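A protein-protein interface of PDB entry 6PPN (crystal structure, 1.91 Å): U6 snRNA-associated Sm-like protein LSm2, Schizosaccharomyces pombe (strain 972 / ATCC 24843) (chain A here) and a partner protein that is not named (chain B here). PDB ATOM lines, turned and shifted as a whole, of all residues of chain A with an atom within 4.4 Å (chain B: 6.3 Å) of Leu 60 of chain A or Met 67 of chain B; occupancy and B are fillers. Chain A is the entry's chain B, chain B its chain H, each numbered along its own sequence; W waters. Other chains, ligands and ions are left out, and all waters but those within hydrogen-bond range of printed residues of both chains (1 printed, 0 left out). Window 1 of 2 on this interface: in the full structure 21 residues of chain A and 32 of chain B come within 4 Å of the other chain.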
ATOM      1  N   LEU A  19     -22.655 -17.356  22.948  1.00  0.00           N
ATOM      2  CA  LEU A  19     -22.330 -16.530  24.106  1.00  0.00           C
ATOM      3  C   LEU A  19     -23.318 -16.803  25.231  1.00  0.00           C
ATOM      4  O   LEU A  19     -24.386 -17.376  25.038  1.00  0.00           O
ATOM      5  CB  LEU A  19     -22.351 -15.041  23.740  1.00  0.00           C
ATOM      6  CG  LEU A  19     -21.251 -14.443  22.854  1.00  0.00           C
ATOM      7  CD1 LEU A  19     -21.296 -14.962  21.464  1.00  0.00           C
ATOM      8  CD2 LEU A  19     -21.522 -12.965  22.778  1.00  0.00           C
ATOM      9  N   ASN A  21     -25.223 -14.758  26.586  1.00  0.00           N
ATOM     10  CA  ASN A  21     -26.502 -14.068  26.406  1.00  0.00           C
ATOM     11  C   ASN A  21     -27.338 -14.715  25.326  1.00  0.00           C
ATOM     12  O   ASN A  21     -28.268 -14.091  24.820  1.00  0.00           O
ATOM     13  CB  ASN A  21     -26.308 -12.575  26.097  1.00  0.00           C
ATOM     14  CG  ASN A  21     -25.517 -12.330  24.835  1.00  0.00           C
ATOM     15  OD1 ASN A  21     -25.204 -13.259  24.099  1.00  0.00           O
ATOM     16  ND2 ASN A  21     -25.187 -11.066  24.574  1.00  0.00           N
ATOM     17  N   MET A  23     -26.843 -15.236  22.243  1.00  0.00           N
ATOM     18  CA  MET A  23     -26.426 -14.939  20.878  1.00  0.00           C
ATOM     19  C   MET A  23     -25.332 -15.890  20.427  1.00  0.00           C
ATOM     20  O   MET A  23     -24.450 -16.284  21.198  1.00  0.00           O
ATOM     21  CB  MET A  23     -25.902 -13.501  20.746  1.00  0.00           C
ATOM     22  CG  MET A  23     -26.951 -12.459  21.076  1.00  0.00           C
ATOM     23  SD  MET A  23     -26.329 -10.765  20.804  1.00  0.00           S
ATOM     24  CE  MET A  23     -25.852 -10.862  19.077  1.00  0.00           C
ATOM     25  N   ILE A  25     -22.498 -16.223  17.116  1.00  0.00           N
ATOM     26  CA  ILE A  25     -21.864 -15.499  16.028  1.00  0.00           C
ATOM     27  C   ILE A  25     -20.933 -16.431  15.258  1.00  0.00           C
ATOM     28  O   ILE A  25     -20.088 -17.112  15.856  1.00  0.00           O
ATOM     29  CB  ILE A  25     -21.124 -14.264  16.559  1.00  0.00           C
ATOM     30  CG1 ILE A  25     -22.179 -13.295  17.108  1.00  0.00           C
ATOM     31  CG2 ILE A  25     -20.396 -13.576  15.429  1.00  0.00           C
ATOM     32  CD1 ILE A  25     -21.775 -12.616  18.311  1.00  0.00           C
ATOM     33  N   VAL A  38     -11.456 -13.661  21.800  1.00  0.00           N
ATOM     34  CA  VAL A  38     -11.394 -14.173  20.438  1.00  0.00           C
ATOM     35  C   VAL A  38     -11.750 -13.057  19.442  1.00  0.00           C
ATOM     36  O   VAL A  38     -12.506 -12.136  19.772  1.00  0.00           O
ATOM     37  CB  VAL A  38     -12.305 -15.423  20.441  1.00  0.00           C
ATOM     38  CG1 VAL A  38     -13.694 -15.197  19.878  1.00  0.00           C
ATOM     39  CG2 VAL A  38     -11.593 -16.658  19.980  1.00  0.00           C
ATOM     40  N   LYS A  39     -11.091 -13.028  18.286  1.00  0.00           N
ATOM     41  CA  LYS A  39     -11.466 -12.070  17.246  1.00  0.00           C
ATOM     42  C   LYS A  39     -11.959 -12.830  16.030  1.00  0.00           C
ATOM     43  O   LYS A  39     -11.239 -13.682  15.506  1.00  0.00           O
ATOM     44  CB  LYS A  39     -10.315 -11.175  16.803  1.00  0.00           C
ATOM     45  CG  LYS A  39     -10.785 -10.171  15.730  1.00  0.00           C
ATOM     46  CD  LYS A  39      -9.672  -9.229  15.313  1.00  0.00           C
ATOM     47  CE  LYS A  39     -10.051  -8.405  14.092  1.00  0.00           C
ATOM     48  NZ  LYS A  39      -8.869  -7.854  13.335  1.00  0.00           N
ATOM     49  N   LEU A  40     -13.160 -12.512  15.573  1.00  0.00           N
ATOM     50  CA  LEU A  40     -13.766 -13.153  14.417  1.00  0.00           C
ATOM     51  C   LEU A  40     -13.867 -12.120  13.303  1.00  0.00           C
ATOM     52  O   LEU A  40     -14.042 -10.928  13.565  1.00  0.00           O
ATOM     53  CB  LEU A  40     -15.147 -13.702  14.746  1.00  0.00           C
ATOM     54  CG  LEU A  40     -15.303 -14.632  15.952  1.00  0.00           C
ATOM     55  CD1 LEU A  40     -16.749 -15.064  16.057  1.00  0.00           C
ATOM     56  CD2 LEU A  40     -14.430 -15.850  15.768  1.00  0.00           C
ATOM     57  N   ILE A  43     -18.126 -11.664  10.295  1.00  0.00           N
ATOM     58  CA  ILE A  43     -19.099 -12.365  11.111  1.00  0.00           C
ATOM     59  C   ILE A  43     -20.490 -12.231  10.507  1.00  0.00           C
ATOM     60  O   ILE A  43     -20.808 -11.258   9.809  1.00  0.00           O
ATOM     61  CB  ILE A  43     -19.074 -11.822  12.548  1.00  0.00           C
ATOM     62  CG1 ILE A  43     -19.555 -10.374  12.562  1.00  0.00           C
ATOM     63  CG2 ILE A  43     -17.670 -11.911  13.107  1.00  0.00           C
ATOM     64  CD1 ILE A  43     -20.875 -10.173  13.295  1.00  0.00           C
ATOM     65  N   MET A  54     -26.044  -5.820  14.561  1.00  0.00           N
ATOM     66  CA  MET A  54     -24.677  -5.973  14.096  1.00  0.00           C
ATOM     67  C   MET A  54     -24.590  -6.047  12.585  1.00  0.00           C
ATOM     68  O   MET A  54     -23.606  -6.568  12.039  1.00  0.00           O
ATOM     69  CB  MET A  54     -24.080  -7.209  14.755  1.00  0.00           C
ATOM     70  CG  MET A  54     -24.470  -7.227  16.218  1.00  0.00           C
ATOM     71  SD  MET A  54     -23.241  -7.936  17.270  1.00  0.00           S
ATOM     72  CE  MET A  54     -21.732  -7.159  16.703  1.00  0.00           C
ATOM     73  N   LYS A  58     -18.435  -6.203  10.695  1.00  0.00           N
ATOM     74  CA  LYS A  58     -17.796  -7.335  10.042  1.00  0.00           C
ATOM     75  C   LYS A  58     -16.757  -8.009  10.921  1.00  0.00           C
ATOM     76  O   LYS A  58     -16.677  -9.246  10.944  1.00  0.00           O
ATOM     77  CB  LYS A  58     -17.157  -6.889   8.717  1.00  0.00           C
ATOM     78  N   ASP A  59     -15.972  -7.231  11.662  1.00  0.00           N
ATOM     79  CA  ASP A  59     -14.950  -7.745  12.562  1.00  0.00           C
ATOM     80  C   ASP A  59     -15.398  -7.556  14.000  1.00  0.00           C
ATOM     81  O   ASP A  59     -15.960  -6.515  14.352  1.00  0.00           O
ATOM     82  CB  ASP A  59     -13.622  -7.037  12.342  1.00  0.00           C
ATOM     83  CG  ASP A  59     -13.101  -7.234  10.954  1.00  0.00           C
ATOM     84  OD1 ASP A  59     -13.731  -8.002  10.190  1.00  0.00           O
ATOM     85  OD2 ASP A  59     -12.061  -6.630  10.636  1.00  0.00           O
ATOM     86  N   LEU A  60     -15.156  -8.570  14.828  1.00  0.00           N
ATOM     87  CA  LEU A  60     -15.796  -8.636  16.130  1.00  0.00           C
ATOM     88  C   LEU A  60     -14.834  -9.189  17.153  1.00  0.00           C
ATOM     89  O   LEU A  60     -14.226 -10.235  16.926  1.00  0.00           O
ATOM     90  CB  LEU A  60     -17.034  -9.514  16.086  1.00  0.00           C
ATOM     91  CG  LEU A  60     -17.741  -9.620  17.432  1.00  0.00           C
ATOM     92  CD1 LEU A  60     -18.349  -8.265  17.786  1.00  0.00           C
ATOM     93  CD2 LEU A  60     -18.827 -10.702  17.366  1.00  0.00           C
ATOM     94  N   PHE A  61     -14.713  -8.495  18.279  1.00  0.00           N
ATOM     95  CA  PHE A  61     -14.000  -8.988  19.450  1.00  0.00           C
ATOM     96  C   PHE A  61     -14.994  -9.528  20.461  1.00  0.00           C
ATOM     97  O   PHE A  61     -15.973  -8.851  20.799  1.00  0.00           O
ATOM     98  CB  PHE A  61     -13.169  -7.858  20.049  1.00  0.00           C
ATOM     99  CG  PHE A  61     -12.551  -8.173  21.383  1.00  0.00           C
ATOM    100  CD1 PHE A  61     -13.292  -8.100  22.546  1.00  0.00           C
ATOM    101  CD2 PHE A  61     -11.207  -8.481  21.473  1.00  0.00           C
ATOM    102  CE1 PHE A  61     -12.701  -8.355  23.779  1.00  0.00           C
ATOM    103  CE2 PHE A  61     -10.609  -8.726  22.706  1.00  0.00           C
ATOM    104  CZ  PHE A  61     -11.367  -8.675  23.842  1.00  0.00           C
ATOM    105  N   ILE A  62     -14.746 -10.737  20.960  1.00  0.00           N
ATOM    106  CA  ILE A  62     -15.604 -11.355  21.962  1.00  0.00           C
ATOM    107  C   ILE A  62     -14.773 -11.607  23.209  1.00  0.00           C
ATOM    108  O   ILE A  62     -13.722 -12.247  23.131  1.00  0.00           O
ATOM    109  CB  ILE A  62     -16.185 -12.679  21.447  1.00  0.00           C
ATOM    110  CG1 ILE A  62     -16.875 -12.459  20.108  1.00  0.00           C
ATOM    111  CG2 ILE A  62     -17.148 -13.272  22.499  1.00  0.00           C
ATOM    112  CD1 ILE A  62     -17.502 -13.743  19.528  1.00  0.00           C
ATOM    113  N   PHE B   6      -8.736  -2.060  16.505  1.00  0.00           N
ATOM    114  CA  PHE B   6      -9.885  -1.161  16.443  1.00  0.00           C
ATOM    115  C   PHE B   6      -9.586   0.256  16.935  1.00  0.00           C
ATOM    116  O   PHE B   6     -10.496   1.094  16.932  1.00  0.00           O
ATOM    117  CB  PHE B   6     -11.045  -1.716  17.273  1.00  0.00           C
ATOM    118  CG  PHE B   6     -11.565  -3.044  16.811  1.00  0.00           C
ATOM    119  CD1 PHE B   6     -11.277  -3.527  15.556  1.00  0.00           C
ATOM    120  CD2 PHE B   6     -12.374  -3.805  17.652  1.00  0.00           C
ATOM    121  CE1 PHE B   6     -11.774  -4.750  15.139  1.00  0.00           C
ATOM    122  CE2 PHE B   6     -12.886  -5.027  17.243  1.00  0.00           C
ATOM    123  CZ  PHE B   6     -12.572  -5.509  15.972  1.00  0.00           C
ATOM    124  N   GLN B  12     -18.650  -0.626  18.267  1.00  0.00           N
ATOM    125  CA  GLN B  12     -19.974  -0.848  18.837  1.00  0.00           C
ATOM    126  C   GLN B  12     -19.852  -1.897  19.929  1.00  0.00           C
ATOM    127  O   GLN B  12     -19.539  -3.050  19.650  1.00  0.00           O
ATOM    128  CB  GLN B  12     -20.993  -1.298  17.787  1.00  0.00           C
ATOM    129  CG  GLN B  12     -22.293  -1.829  18.428  1.00  0.00           C
ATOM    130  CD  GLN B  12     -23.394  -2.131  17.422  1.00  0.00           C
ATOM    131  OE1 GLN B  12     -23.985  -1.220  16.840  1.00  0.00           O
ATOM    132  NE2 GLN B  12     -23.675  -3.417  17.216  1.00  0.00           N
ATOM    133  N   VAL B  13     -20.135  -1.511  21.165  1.00  0.00           N
ATOM    134  CA  VAL B  13     -19.938  -2.371  22.322  1.00  0.00           C
ATOM    135  C   VAL B  13     -21.281  -2.928  22.730  1.00  0.00           C
ATOM    136  O   VAL B  13     -22.257  -2.174  22.855  1.00  0.00           O
ATOM    137  CB  VAL B  13     -19.322  -1.599  23.502  1.00  0.00           C
ATOM    138  CG1 VAL B  13     -19.208  -2.542  24.703  1.00  0.00           C
ATOM    139  CG2 VAL B  13     -17.943  -1.021  23.133  1.00  0.00           C
ATOM    140  N   ILE B  14     -21.333  -4.239  22.940  1.00  0.00           N
ATOM    141  CA  ILE B  14     -22.472  -4.898  23.559  1.00  0.00           C
ATOM    142  C   ILE B  14     -22.044  -5.273  24.966  1.00  0.00           C
ATOM    143  O   ILE B  14     -21.056  -6.005  25.136  1.00  0.00           O
ATOM    144  CB  ILE B  14     -22.904  -6.154  22.798  1.00  0.00           C
ATOM    145  CG1 ILE B  14     -23.057  -5.844  21.324  1.00  0.00           C
ATOM    146  CG2 ILE B  14     -24.209  -6.652  23.371  1.00  0.00           C
ATOM    147  CD1 ILE B  14     -24.248  -5.128  21.072  1.00  0.00           C
ATOM    148  N   THR B  15     -22.790  -4.804  25.961  1.00  0.00           N
ATOM    149  CA  THR B  15     -22.456  -5.032  27.356  1.00  0.00           C
ATOM    150  C   THR B  15     -23.267  -6.188  27.921  1.00  0.00           C
ATOM    151  O   THR B  15     -24.207  -6.701  27.291  1.00  0.00           O
ATOM    152  CB  THR B  15     -22.708  -3.764  28.163  1.00  0.00           C
ATOM    153  OG1 THR B  15     -24.064  -3.398  28.016  1.00  0.00           O
ATOM    154  CG2 THR B  15     -21.920  -2.639  27.615  1.00  0.00           C
ATOM    155  N   ASN B  16     -22.885  -6.613  29.134  1.00  0.00           N
ATOM    156  CA  ASN B  16     -23.532  -7.781  29.723  1.00  0.00           C
ATOM    157  C   ASN B  16     -24.992  -7.530  30.057  1.00  0.00           C
ATOM    158  O   ASN B  16     -25.753  -8.499  30.179  1.00  0.00           O
ATOM    159  CB  ASN B  16     -22.781  -8.243  30.973  1.00  0.00           C
ATOM    160  CG  ASN B  16     -21.435  -8.885  30.638  1.00  0.00           C
ATOM    161  OD1 ASN B  16     -21.018  -8.924  29.472  1.00  0.00           O
ATOM    162  ND2 ASN B  16     -20.769  -9.424  31.651  1.00  0.00           N
ATOM    163  N   LEU B  34     -12.551  -0.132  28.648  1.00  0.00           N
ATOM    164  CA  LEU B  34     -12.517   0.588  27.378  1.00  0.00           C
ATOM    165  C   LEU B  34     -12.781   2.062  27.632  1.00  0.00           C
ATOM    166  O   LEU B  34     -13.502   2.413  28.566  1.00  0.00           O
ATOM    167  CB  LEU B  34     -13.574   0.088  26.388  1.00  0.00           C
ATOM    168  CG  LEU B  34     -13.686  -1.410  26.161  1.00  0.00           C
ATOM    169  CD1 LEU B  34     -14.910  -1.670  25.305  1.00  0.00           C
ATOM    170  CD2 LEU B  34     -12.446  -1.952  25.470  1.00  0.00           C
ATOM    171  N   VAL B  65     -18.199  -5.957  29.589  1.00  0.00           N
ATOM    172  CA  VAL B  65     -18.094  -5.938  28.133  1.00  0.00           C
ATOM    173  C   VAL B  65     -18.249  -7.353  27.601  1.00  0.00           C
ATOM    174  O   VAL B  65     -17.497  -8.260  27.979  1.00  0.00           O
ATOM    175  CB  VAL B  65     -16.751  -5.347  27.688  1.00  0.00           C
ATOM    176  CG1 VAL B  65     -16.574  -5.540  26.173  1.00  0.00           C
ATOM    177  CG2 VAL B  65     -16.701  -3.876  28.047  1.00  0.00           C
ATOM    178  N   ALA B  66     -19.226  -7.549  26.722  1.00  0.00           N
ATOM    179  CA  ALA B  66     -19.384  -8.828  26.038  1.00  0.00           C
ATOM    180  C   ALA B  66     -18.706  -8.831  24.680  1.00  0.00           C
ATOM    181  O   ALA B  66     -17.938  -9.746  24.356  1.00  0.00           O
ATOM    182  CB  ALA B  66     -20.882  -9.165  25.867  1.00  0.00           C
ATOM    183  N   MET B  67     -18.980  -7.834  23.860  1.00  0.00           N
ATOM    184  CA  MET B  67     -18.448  -7.840  22.502  1.00  0.00           C
ATOM    185  C   MET B  67     -18.055  -6.439  22.146  1.00  0.00           C
ATOM    186  O   MET B  67     -18.722  -5.500  22.572  1.00  0.00           O
ATOM    187  CB  MET B  67     -19.484  -8.270  21.461  1.00  0.00           C
ATOM    188  CG  MET B  67     -19.816  -9.728  21.475  1.00  0.00           C
ATOM    189  SD  MET B  67     -21.210  -9.899  20.366  1.00  0.00           S
ATOM    190  CE  MET B  67     -22.575  -9.812  21.529  1.00  0.00           C
ATOM    191  N   VAL B  68     -17.026  -6.309  21.309  1.00  0.00           N
ATOM    192  CA  VAL B  68     -16.658  -5.036  20.680  1.00  0.00           C
ATOM    193  C   VAL B  68     -16.593  -5.260  19.169  1.00  0.00           C
ATOM    194  O   VAL B  68     -15.736  -6.005  18.687  1.00  0.00           O
ATOM    195  CB  VAL B  68     -15.315  -4.496  21.199  1.00  0.00           C
ATOM    196  CG1 VAL B  68     -15.012  -3.150  20.555  1.00  0.00           C
ATOM    197  CG2 VAL B  68     -15.318  -4.378  22.740  1.00  0.00           C
ATOM    198  N   GLY B  69     -17.497  -4.641  18.422  1.00  0.00           N
ATOM    199  CA  GLY B  69     -17.547  -4.789  16.976  1.00  0.00           C
ATOM    200  C   GLY B  69     -17.008  -3.539  16.303  1.00  0.00           C
ATOM    201  O   GLY B  69     -17.216  -2.438  16.788  1.00  0.00           O
ATOM    202  N   LEU B  70     -16.311  -3.713  15.188  1.00  0.00           N
ATOM    203  CA  LEU B  70     -15.826  -2.586  14.409  1.00  0.00           C
ATOM    204  C   LEU B  70     -16.934  -2.200  13.439  1.00  0.00           C
ATOM    205  O   LEU B  70     -17.368  -3.034  12.638  1.00  0.00           O
ATOM    206  CB  LEU B  70     -14.551  -2.976  13.662  1.00  0.00           C
ATOM    207  CG  LEU B  70     -13.833  -1.904  12.857  1.00  0.00           C
ATOM    208  CD1 LEU B  70     -13.194  -0.897  13.802  1.00  0.00           C
ATOM    209  CD2 LEU B  70     -12.749  -2.548  12.021  1.00  0.00           C
ATOM    210  N   ILE B  89     -31.458  -7.201  23.294  1.00  0.00           N
ATOM    211  CA  ILE B  89     -30.409  -8.208  23.486  1.00  0.00           C
ATOM    212  C   ILE B  89     -30.483  -8.742  24.915  1.00  0.00           C
ATOM    213  O   ILE B  89     -30.629  -7.947  25.866  1.00  0.00           O
ATOM    214  CB  ILE B  89     -29.039  -7.603  23.177  1.00  0.00           C
ATOM    215  CG1 ILE B  89     -29.009  -7.148  21.715  1.00  0.00           C
ATOM    216  CG2 ILE B  89     -27.927  -8.593  23.480  1.00  0.00           C
ATOM    217  CD1 ILE B  89     -27.644  -6.724  21.232  1.00  0.00           C
HETATM  218  O   HOH W   1     -25.755  -9.192  26.421  1.00  0.00           O
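Among the printed residues, merely in contact across the chains: Phe 61 of chain A with Met 67 of chain B (3.2 Å), Ile 25 of chain A with Met 67 of chain B (3.5 Å), Asp 59 of chain A with Gly 69 of chain B (3.5 Å), Leu 19 of chain A with Met 67 of chain B (3.6 Å), Leu 60 of chain A with Val 68 of chain B (3.6 Å), Leu 60 of chain A with Gly 69 of chain B (3.7 Å), Ile 62 of chain A with Ala 66 of chain B (3.7 Å), Met 23 of chain A with Ile 89 of chain B (3.8 Å), Leu 60 of chain A with Met 67 of chain B (3.8 Å), Asn 21 of chain A with Ile 89 of chain B (3.8 Å), Lys 58 of chain A with Leu 70 of chain B (3.9 Å), Asp 59 of chain A with Phe 6 of chain B (3.9 Å), Met 23 of chain A with Met 67 of chain B (3.9 Å) and Phe 61 of chain A with Phe 6 of chain B (3.996 Å).
Along chain A the printed residues that touch a printed residue of chain B span positions 19 to 62. Hydrophobic or aromatic side chains of chain B that line the printed part of chain A: Phe 6, Met 67, Leu 70 and Ile 89. Along chain B the printed residues that touch a printed residue of chain A span positions 6 to 89. Among the printed residues, 16 pairs touch across the chains. Among the printed residues, no Asp or Glu carboxylate lies within 4 Å of a Lys or Arg side-chain nitrogen of the other chain.
Water W1 lies within hydrogen-bond range of ND2 of Asn 21 of chain A (2.7 Å) and O of Thr 15 of chain B (3.1 Å).
The backbone carbonyl oxygen (O) of Asp 59 of chain A sits at hydrogen-bond distance from the backbone NH (N) of Leu 70 of chain B, 2.9 Å away. The backbone NH (N) of Phe 61 of chain A is in hydrogen-bond range of the backbone carbonyl oxygen (O) of Val 68 of chain B (2.7 Å).
The backbone NH (N) of Leu 40 of chain A is in hydrogen-bond range of the backbone carbonyl oxygen (O) of Leu 60 of chain A, 2.9 Å away. The backbone carbonyl oxygen (O) of Ile 14 of chain B lies within hydrogen-bond range of the backbone NH (N) of Ala 66 of chain B. N of Ile 62 of chain A is in hydrogen-bond range of O of Val 38 of chain A (2.9 Å). The backbone NH of Ile 43 of chain A is in hydrogen-bond range of the backbone carbonyl oxygen of Lys 58 of chain A. The backbone NH of Ile 14 of chain B is in hydrogen-bond range of the backbone carbonyl oxygen of Met 67 of chain B, 2.9 Å away. The backbone carbonyl oxygen (O) of Gly 69 of chain B lies within hydrogen-bond range of the backbone NH (N) of Gln 12 of chain B (2.7 Å).
Leu 60 of chain A touches three residues of chain B. Of chain A, only Leu 19 (3.6 Å), Met 23 (3.9 Å), Ile 25 (3.5 Å), Leu 60 (3.8 Å) and Phe 61 (3.2 Å) come within 4 Å of Met 67 of chain B. Printed residues of chain B within 4 Å of Leu 19 of chain A: Met 67. Of the printed residues of chain B, Phe 61 of chain A touches Phe 6, Met 67 and Val 68. Printed residues of chain B within 4 Å of Ile 62 of chain A: Ala 66. Of the printed residues of chain B, Asp 59 of chain A touches Phe 6 (3.9 Å), Gly 69 (3.5 Å) and Leu 70 (2.9 Å). Ile 43 of chain A touches none of the printed residues of chain B. The nearest printed residue of chain B that does not touch Met 23 of chain A is Ile 14 of chain B (5.3 Å).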
